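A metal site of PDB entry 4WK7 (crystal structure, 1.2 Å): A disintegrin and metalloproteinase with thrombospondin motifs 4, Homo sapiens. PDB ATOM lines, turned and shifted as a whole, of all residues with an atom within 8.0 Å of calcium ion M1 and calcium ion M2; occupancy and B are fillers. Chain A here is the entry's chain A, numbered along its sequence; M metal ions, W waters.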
ATOM      1  N   PHE A   7     -27.625   9.726 -18.544  1.00  0.00           N
ATOM      2  CA  PHE A   7     -28.710  10.032 -17.611  1.00  0.00           C
ATOM      3  C   PHE A   7     -28.159  10.735 -16.391  1.00  0.00           C
ATOM      4  O   PHE A   7     -27.204  10.268 -15.776  1.00  0.00           O
ATOM      5  CB  PHE A   7     -29.409   8.732 -17.180  1.00  0.00           C
ATOM      6  CG  PHE A   7     -29.848   7.877 -18.331  1.00  0.00           C
ATOM      7  CD1 PHE A   7     -31.071   8.090 -18.947  1.00  0.00           C
ATOM      8  CD2 PHE A   7     -29.023   6.862 -18.813  1.00  0.00           C
ATOM      9  CE1 PHE A   7     -31.469   7.300 -20.017  1.00  0.00           C
ATOM     10  CE2 PHE A   7     -29.429   6.070 -19.871  1.00  0.00           C
ATOM     11  CZ  PHE A   7     -30.647   6.288 -20.475  1.00  0.00           C
ATOM     12  N   VAL A   8     -28.750  11.880 -16.051  1.00  0.00           N
ATOM     13  CA  VAL A   8     -28.381  12.602 -14.846  1.00  0.00           C
ATOM     14  C   VAL A   8     -29.438  12.344 -13.783  1.00  0.00           C
ATOM     15  O   VAL A   8     -30.555  12.853 -13.876  1.00  0.00           O
ATOM     16  CB  VAL A   8     -28.277  14.118 -15.080  1.00  0.00           C
ATOM     17  CG1 VAL A   8     -27.631  14.799 -13.886  1.00  0.00           C
ATOM     18  CG2 VAL A   8     -27.478  14.414 -16.342  1.00  0.00           C
ATOM     19  N   GLU A   9     -29.089  11.514 -12.793  1.00  0.00           N
ATOM     20  CA  GLU A   9     -30.006  11.205 -11.706  1.00  0.00           C
ATOM     21  C   GLU A   9     -30.023  12.390 -10.753  1.00  0.00           C
ATOM     22  O   GLU A   9     -29.024  12.705 -10.107  1.00  0.00           O
ATOM     23  CB  GLU A   9     -29.566   9.913 -11.006  1.00  0.00           C
ATOM     24  CG  GLU A   9     -29.628   8.705 -11.931  1.00  0.00           C
ATOM     25  CD  GLU A   9     -28.965   7.483 -11.332  1.00  0.00           C
ATOM     26  OE1 GLU A   9     -27.720   7.479 -11.205  1.00  0.00           O
ATOM     27  OE2 GLU A   9     -29.656   6.515 -10.972  1.00  0.00           O
ATOM     28  N   THR A  10     -31.151  13.078 -10.699  1.00  0.00           N
ATOM     29  CA  THR A  10     -31.203  14.402 -10.089  1.00  0.00           C
ATOM     30  C   THR A  10     -32.030  14.430  -8.811  1.00  0.00           C
ATOM     31  O   THR A  10     -33.180  13.986  -8.794  1.00  0.00           O
ATOM     32  CB  THR A  10     -31.764  15.428 -11.089  1.00  0.00           C
ATOM     33  OG1 THR A  10     -31.009  15.369 -12.300  1.00  0.00           O
ATOM     34  CG2 THR A  10     -31.717  16.842 -10.521  1.00  0.00           C
ATOM     35  N   THR A  55     -35.008  11.904  -9.795  1.00  0.00           N
ATOM     36  CA  THR A  55     -35.097  10.620  -9.095  1.00  0.00           C
ATOM     37  C   THR A  55     -35.463  10.777  -7.620  1.00  0.00           C
ATOM     38  O   THR A  55     -36.012   9.848  -7.030  1.00  0.00           O
ATOM     39  CB  THR A  55     -33.787   9.824  -9.230  1.00  0.00           C
ATOM     40  OG1 THR A  55     -32.685  10.618  -8.768  1.00  0.00           O
ATOM     41  CG2 THR A  55     -33.555   9.431 -10.671  1.00  0.00           C
ATOM     42  N   THR A  89     -25.597   8.433  -1.196  1.00  0.00           N
ATOM     43  CA  THR A  89     -24.959   7.165  -0.825  1.00  0.00           C
ATOM     44  C   THR A  89     -23.595   7.088  -1.518  1.00  0.00           C
ATOM     45  O   THR A  89     -23.360   7.787  -2.501  1.00  0.00           O
ATOM     46  CB  THR A  89     -25.801   5.969  -1.262  1.00  0.00           C
ATOM     47  OG1 THR A  89     -25.910   5.943  -2.696  1.00  0.00           O
ATOM     48  CG2 THR A  89     -27.198   6.040  -0.659  1.00  0.00           C
ATOM     49  N   GLU A  91     -22.256   4.756  -3.434  1.00  0.00           N
ATOM     50  CA  GLU A  91     -22.189   4.055  -4.720  1.00  0.00           C
ATOM     51  C   GLU A  91     -23.363   4.371  -5.632  1.00  0.00           C
ATOM     52  O   GLU A  91     -24.520   4.371  -5.205  1.00  0.00           O
ATOM     53  CB  GLU A  91     -22.105   2.549  -4.491  1.00  0.00           C
ATOM     54  CG  GLU A  91     -20.901   2.105  -3.671  1.00  0.00           C
ATOM     55  CD  GLU A  91     -19.574   2.410  -4.332  1.00  0.00           C
ATOM     56  OE1 GLU A  91     -19.546   2.635  -5.561  1.00  0.00           O
ATOM     57  OE2 GLU A  91     -18.547   2.435  -3.620  1.00  0.00           O
ATOM     58  N   ASP A  92     -23.058   4.610  -6.914  1.00  0.00           N
ATOM     59  CA  ASP A  92     -24.075   4.959  -7.908  1.00  0.00           C
ATOM     60  C   ASP A  92     -25.033   3.799  -8.191  1.00  0.00           C
ATOM     61  O   ASP A  92     -26.154   4.010  -8.638  1.00  0.00           O
ATOM     62  CB  ASP A  92     -23.399   5.443  -9.200  1.00  0.00           C
ATOM     63  CG  ASP A  92     -24.268   6.368 -10.041  1.00  0.00           C
ATOM     64  OD1 ASP A  92     -25.463   6.587  -9.756  1.00  0.00           O
ATOM     65  OD2 ASP A  92     -23.738   6.901 -11.039  1.00  0.00           O
ATOM     66  N   SER A  93     -24.610   2.564  -7.914  1.00  0.00           N
ATOM     67  CA  SER A  93     -25.499   1.404  -8.080  1.00  0.00           C
ATOM     68  C   SER A  93     -26.609   1.306  -7.030  1.00  0.00           C
ATOM     69  O   SER A  93     -27.581   0.586  -7.224  1.00  0.00           O
ATOM     70  CB  SER A  93     -24.687   0.107  -8.106  1.00  0.00           C
ATOM     71  OG  SER A  93     -23.950  -0.056  -6.913  1.00  0.00           O
ATOM     72  N   ASP A  94     -26.465   2.028  -5.911  1.00  0.00           N
ATOM     73  CA  ASP A  94     -27.538   2.130  -4.927  1.00  0.00           C
ATOM     74  C   ASP A  94     -28.636   3.019  -5.520  1.00  0.00           C
ATOM     75  O   ASP A  94     -28.331   4.122  -5.974  1.00  0.00           O
ATOM     76  CB  ASP A  94     -26.992   2.746  -3.637  1.00  0.00           C
ATOM     77  CG  ASP A  94     -28.010   2.761  -2.508  1.00  0.00           C
ATOM     78  OD1 ASP A  94     -29.145   3.233  -2.716  1.00  0.00           O
ATOM     79  OD2 ASP A  94     -27.656   2.316  -1.400  1.00  0.00           O
ATOM     80  N   PRO A  95     -29.903   2.567  -5.522  1.00  0.00           N
ATOM     81  CA  PRO A  95     -30.943   3.383  -6.172  1.00  0.00           C
ATOM     82  C   PRO A  95     -31.165   4.764  -5.538  1.00  0.00           C
ATOM     83  O   PRO A  95     -31.661   5.663  -6.225  1.00  0.00           O
ATOM     84  CB  PRO A  95     -32.208   2.529  -6.036  1.00  0.00           C
ATOM     85  CG  PRO A  95     -31.935   1.631  -4.886  1.00  0.00           C
ATOM     86  CD  PRO A  95     -30.465   1.338  -4.935  1.00  0.00           C
ATOM     87  N   ASP A  96     -30.784   4.946  -4.269  1.00  0.00           N
ATOM     88  CA  ASP A  96     -30.897   6.252  -3.608  1.00  0.00           C
ATOM     89  C   ASP A  96     -29.805   7.230  -4.041  1.00  0.00           C
ATOM     90  O   ASP A  96     -29.908   8.429  -3.748  1.00  0.00           O
ATOM     91  CB  ASP A  96     -30.831   6.106  -2.085  1.00  0.00           C
ATOM     92  CG  ASP A  96     -32.019   5.370  -1.505  1.00  0.00           C
ATOM     93  OD1 ASP A  96     -33.038   5.181  -2.204  1.00  0.00           O
ATOM     94  OD2 ASP A  96     -31.938   4.993  -0.318  1.00  0.00           O
ATOM     95  N   HIS A  97     -28.756   6.752  -4.699  1.00  0.00           N
ATOM     96  CA  HIS A  97     -27.685   7.647  -5.135  1.00  0.00           C
ATOM     97  C   HIS A  97     -28.189   8.605  -6.202  1.00  0.00           C
ATOM     98  O   HIS A  97     -29.003   8.232  -7.050  1.00  0.00           O
ATOM     99  CB  HIS A  97     -26.497   6.864  -5.697  1.00  0.00           C
ATOM    100  CG  HIS A  97     -25.314   7.730  -6.020  1.00  0.00           C
ATOM    101  ND1 HIS A  97     -24.310   7.990  -5.113  1.00  0.00           N
ATOM    102  CD2 HIS A  97     -24.972   8.396  -7.156  1.00  0.00           C
ATOM    103  CE1 HIS A  97     -23.403   8.774  -5.667  1.00  0.00           C
ATOM    104  NE2 HIS A  97     -23.786   9.038  -6.900  1.00  0.00           N
ATOM    105  N   PHE A  98     -27.694   9.834  -6.159  1.00  0.00           N
ATOM    106  CA  PHE A  98     -27.989  10.832  -7.187  1.00  0.00           C
ATOM    107  C   PHE A  98     -26.702  11.469  -7.696  1.00  0.00           C
ATOM    108  O   PHE A  98     -25.696  11.525  -6.980  1.00  0.00           O
ATOM    109  CB  PHE A  98     -28.982  11.880  -6.681  1.00  0.00           C
ATOM    110  CG  PHE A  98     -28.591  12.517  -5.384  1.00  0.00           C
ATOM    111  CD1 PHE A  98     -27.812  13.669  -5.358  1.00  0.00           C
ATOM    112  CD2 PHE A  98     -29.012  11.971  -4.168  1.00  0.00           C
ATOM    113  CE1 PHE A  98     -27.463  14.251  -4.160  1.00  0.00           C
ATOM    114  CE2 PHE A  98     -28.663  12.552  -2.970  1.00  0.00           C
ATOM    115  CZ  PHE A  98     -27.880  13.697  -2.959  1.00  0.00           C
ATOM    116  N   ASP A  99     -26.742  11.931  -8.935  1.00  0.00           N
ATOM    117  CA  ASP A  99     -25.580  12.510  -9.618  1.00  0.00           C
ATOM    118  C   ASP A  99     -25.477  14.028  -9.467  1.00  0.00           C
ATOM    119  O   ASP A  99     -24.392  14.578  -9.609  1.00  0.00           O
ATOM    120  CB  ASP A  99     -25.623  12.195 -11.108  1.00  0.00           C
ATOM    121  CG  ASP A  99     -25.660  10.707 -11.403  1.00  0.00           C
ATOM    122  OD1 ASP A  99     -24.883   9.932 -10.785  1.00  0.00           O
ATOM    123  OD2 ASP A  99     -26.450  10.300 -12.278  1.00  0.00           O
ATOM    124  N   THR A 100     -26.592  14.707  -9.241  1.00  0.00           N
ATOM    125  CA  THR A 100     -26.550  16.155  -9.053  1.00  0.00           C
ATOM    126  C   THR A 100     -27.694  16.583  -8.148  1.00  0.00           C
ATOM    127  O   THR A 100     -28.696  15.864  -8.032  1.00  0.00           O
ATOM    128  CB  THR A 100     -26.560  16.910 -10.403  1.00  0.00           C
ATOM    129  OG1 THR A 100     -25.941  18.193 -10.233  1.00  0.00           O
ATOM    130  CG2 THR A 100     -27.958  17.085 -10.960  1.00  0.00           C
ATOM    131  N   VAL A 126     -20.223  17.539 -12.471  1.00  0.00           N
ATOM    132  CA  VAL A 126     -21.419  16.690 -12.479  1.00  0.00           C
ATOM    133  C   VAL A 126     -21.202  15.307 -11.851  1.00  0.00           C
ATOM    134  O   VAL A 126     -22.135  14.770 -11.240  1.00  0.00           O
ATOM    135  CB  VAL A 126     -22.023  16.561 -13.909  1.00  0.00           C
ATOM    136  CG1 VAL A 126     -21.249  15.577 -14.769  1.00  0.00           C
ATOM    137  CG2 VAL A 126     -23.497  16.146 -13.828  1.00  0.00           C
ATOM    138  N   CYS A 127     -20.008  14.744 -11.963  1.00  0.00           N
ATOM    139  CA  CYS A 127     -19.756  13.421 -11.376  1.00  0.00           C
ATOM    140  C   CYS A 127     -18.854  13.455 -10.159  1.00  0.00           C
ATOM    141  O   CYS A 127     -18.201  12.463  -9.840  1.00  0.00           O
ATOM    142  CB  CYS A 127     -19.226  12.464 -12.451  1.00  0.00           C
ATOM    143  SG  CYS A 127     -20.510  12.028 -13.642  1.00  0.00           S
ATOM    144  N   GLY A 209     -18.086  12.563 -17.346  1.00  0.00           N
ATOM    145  CA  GLY A 209     -19.465  12.101 -17.203  1.00  0.00           C
ATOM    146  C   GLY A 209     -19.597  10.608 -16.935  1.00  0.00           C
ATOM    147  O   GLY A 209     -20.598   9.993 -17.288  1.00  0.00           O
ATOM    148  N   HIS A 210     -18.579  10.031 -16.296  1.00  0.00           N
ATOM    149  CA  HIS A 210     -18.527   8.592 -16.025  1.00  0.00           C
ATOM    150  C   HIS A 210     -19.648   8.077 -15.118  1.00  0.00           C
ATOM    151  O   HIS A 210     -19.947   6.883 -15.123  1.00  0.00           O
ATOM    152  CB  HIS A 210     -17.161   8.210 -15.416  1.00  0.00           C
ATOM    153  CG  HIS A 210     -16.853   8.931 -14.142  1.00  0.00           C
ATOM    154  ND1 HIS A 210     -17.329   8.524 -12.915  1.00  0.00           N
ATOM    155  CD2 HIS A 210     -16.126  10.054 -13.907  1.00  0.00           C
ATOM    156  CE1 HIS A 210     -16.906   9.350 -11.984  1.00  0.00           C
ATOM    157  NE2 HIS A 210     -16.174  10.293 -12.556  1.00  0.00           N
ATOM    158  N   CYS A 211     -20.269   8.971 -14.351  1.00  0.00           N
ATOM    159  CA  CYS A 211     -21.408   8.610 -13.484  1.00  0.00           C
ATOM    160  C   CYS A 211     -22.765   8.743 -14.183  1.00  0.00           C
ATOM    161  O   CYS A 211     -23.799   8.538 -13.548  1.00  0.00           O
ATOM    162  CB  CYS A 211     -21.394   9.489 -12.233  1.00  0.00           C
ATOM    163  SG  CYS A 211     -21.960  11.183 -12.492  1.00  0.00           S
ATOM    164  N   LEU A 212     -22.777   9.072 -15.473  1.00  0.00           N
ATOM    165  CA  LEU A 212     -24.019   9.326 -16.191  1.00  0.00           C
ATOM    166  C   LEU A 212     -24.429   8.165 -17.097  1.00  0.00           C
ATOM    167  O   LEU A 212     -25.324   8.306 -17.928  1.00  0.00           O
ATOM    168  CB  LEU A 212     -23.887  10.601 -17.029  1.00  0.00           C
ATOM    169  CG  LEU A 212     -23.442  11.859 -16.278  1.00  0.00           C
ATOM    170  CD1 LEU A 212     -23.314  13.041 -17.225  1.00  0.00           C
ATOM    171  CD2 LEU A 212     -24.394  12.190 -15.132  1.00  0.00           C
ATOM    172  N   LEU A 213     -23.795   7.008 -16.929  1.00  0.00           N
ATOM    173  CA  LEU A 213     -24.020   5.882 -17.841  1.00  0.00           C
ATOM    174  C   LEU A 213     -25.069   4.895 -17.349  1.00  0.00           C
ATOM    175  O   LEU A 213     -25.612   4.141 -18.152  1.00  0.00           O
ATOM    176  CB  LEU A 213     -22.695   5.145 -18.104  1.00  0.00           C
ATOM    177  CG  LEU A 213     -21.495   6.008 -18.495  1.00  0.00           C
ATOM    178  CD1 LEU A 213     -20.243   5.142 -18.626  1.00  0.00           C
ATOM    179  CD2 LEU A 213     -21.768   6.756 -19.791  1.00  0.00           C
ATOM    180  N   ASP A 214     -25.363   4.878 -16.044  1.00  0.00           N
ATOM    181  CA  ASP A 214     -26.392   3.982 -15.512  1.00  0.00           C
ATOM    182  C   ASP A 214     -27.786   4.585 -15.635  1.00  0.00           C
ATOM    183  O   ASP A 214     -27.990   5.781 -15.448  1.00  0.00           O
ATOM    184  CB  ASP A 214     -26.076   3.549 -14.056  1.00  0.00           C
ATOM    185  CG  ASP A 214     -26.009   4.703 -13.067  1.00  0.00           C
ATOM    186  OD1 ASP A 214     -25.489   5.789 -13.408  1.00  0.00           O
ATOM    187  OD2 ASP A 214     -26.459   4.508 -11.922  1.00  0.00           O
ATOM    188  N   LYS A 215     -28.762   3.747 -15.991  1.00  0.00           N
ATOM    189  CA  LYS A 215     -30.129   4.201 -16.238  1.00  0.00           C
ATOM    190  C   LYS A 215     -30.959   4.078 -14.962  1.00  0.00           C
ATOM    191  O   LYS A 215     -31.025   2.989 -14.384  1.00  0.00           O
ATOM    192  CB  LYS A 215     -30.755   3.389 -17.370  1.00  0.00           C
ATOM    193  CG  LYS A 215     -32.013   4.001 -17.970  1.00  0.00           C
ATOM    194  CD  LYS A 215     -32.429   3.280 -19.238  1.00  0.00           C
ATOM    195  CE  LYS A 215     -33.574   3.990 -19.941  1.00  0.00           C
ATOM    196  NZ  LYS A 215     -33.897   3.379 -21.264  1.00  0.00           N
ATOM    197  N   PRO A 216     -31.571   5.180 -14.498  1.00  0.00           N
ATOM    198  CA  PRO A 216     -32.321   5.132 -13.237  1.00  0.00           C
ATOM    199  C   PRO A 216     -33.575   4.259 -13.319  1.00  0.00           C
ATOM    200  O   PRO A 216     -34.246   4.238 -14.345  1.00  0.00           O
ATOM    201  CB  PRO A 216     -32.715   6.600 -12.982  1.00  0.00           C
ATOM    202  CG  PRO A 216     -32.627   7.252 -14.307  1.00  0.00           C
ATOM    203  CD  PRO A 216     -31.592   6.524 -15.110  1.00  0.00           C
ATOM    204  N   GLU A 217     -33.877   3.576 -12.215  1.00  0.00           N
ATOM    205  CA  GLU A 217     -34.953   2.581 -12.175  1.00  0.00           C
ATOM    206  C   GLU A 217     -36.347   3.194 -12.019  1.00  0.00           C
ATOM    207  O   GLU A 217     -37.322   2.664 -12.544  1.00  0.00           O
ATOM    208  CB  GLU A 217     -34.710   1.602 -11.026  1.00  0.00           C
HETATM  209 CA    CA M   1     -27.527   5.322 -10.090  1.00  0.00          CA
HETATM  210 CA    CA M   2     -25.628   7.942 -12.211  1.00  0.00          CA
HETATM  211  O   HOH W   1     -26.989   8.053 -14.216  1.00  0.00           O
HETATM  212  O   HOH W   2     -28.722   5.712  -8.124  1.00  0.00           O
HETATM  213  O   HOH W   3     -28.864   3.416 -10.402  1.00  0.00           O
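O of Glu 9 is in hydrogen-bond range of N of Thr 100 (3.3 Å).
The side-chain sulfur (SG) of Cys 211 forms a disulfide with the side-chain sulfur (SG) of Cys 127, at 2.0 Å.
Calcium ion M1 is bound by the side-chain carboxylate (OD2) of Asp 214 (2.3 Å), water W2 (2.3 Å), water W3 (2.3 Å), the backbone carbonyl oxygen (O) of Asp 92 (2.4 Å), the side-chain carboxylate (OE1) of Glu 9 (2.4 Å), the side-chain carboxylate (OD1) of Asp 92 (2.4 Å) and the side-chain carboxylate (OE2) of Glu 9 (2.6 Å).
Within 4 Å of calcium ion M1: Glu 9, Asp 92 and Asp 214.
Calcium ion M2 is bound by O of Cys 211, at 2.3 Å.
OE1 of Glu 9 binds calcium ion M2 (2.4 Å).
Water W1 binds calcium ion M2 (2.4 Å).
Calcium ion M2 is bound by OD2 of Asp 92, at 2.5 Å.
OD1 of Asp 214 is bound to calcium ion M2, 2.5 Å away.
The side-chain carboxylate (OD2) of Asp 99 is bound to calcium ion M2 (2.5 Å).
OD1 of Asp 99 binds calcium ion M2 (2.6 Å).
OD1 of Asp 92 is bound to calcium ion M2 (2.8 Å).
Calcium ion M2 has eight donor atoms within binding distance.
The nearest printed residue that does not touch calcium ion M2 is Leu 212 (4.5 Å).
Water W1 bridges O of Phe 7 (2.7 Å) and O of Asp 214 (2.8 Å).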
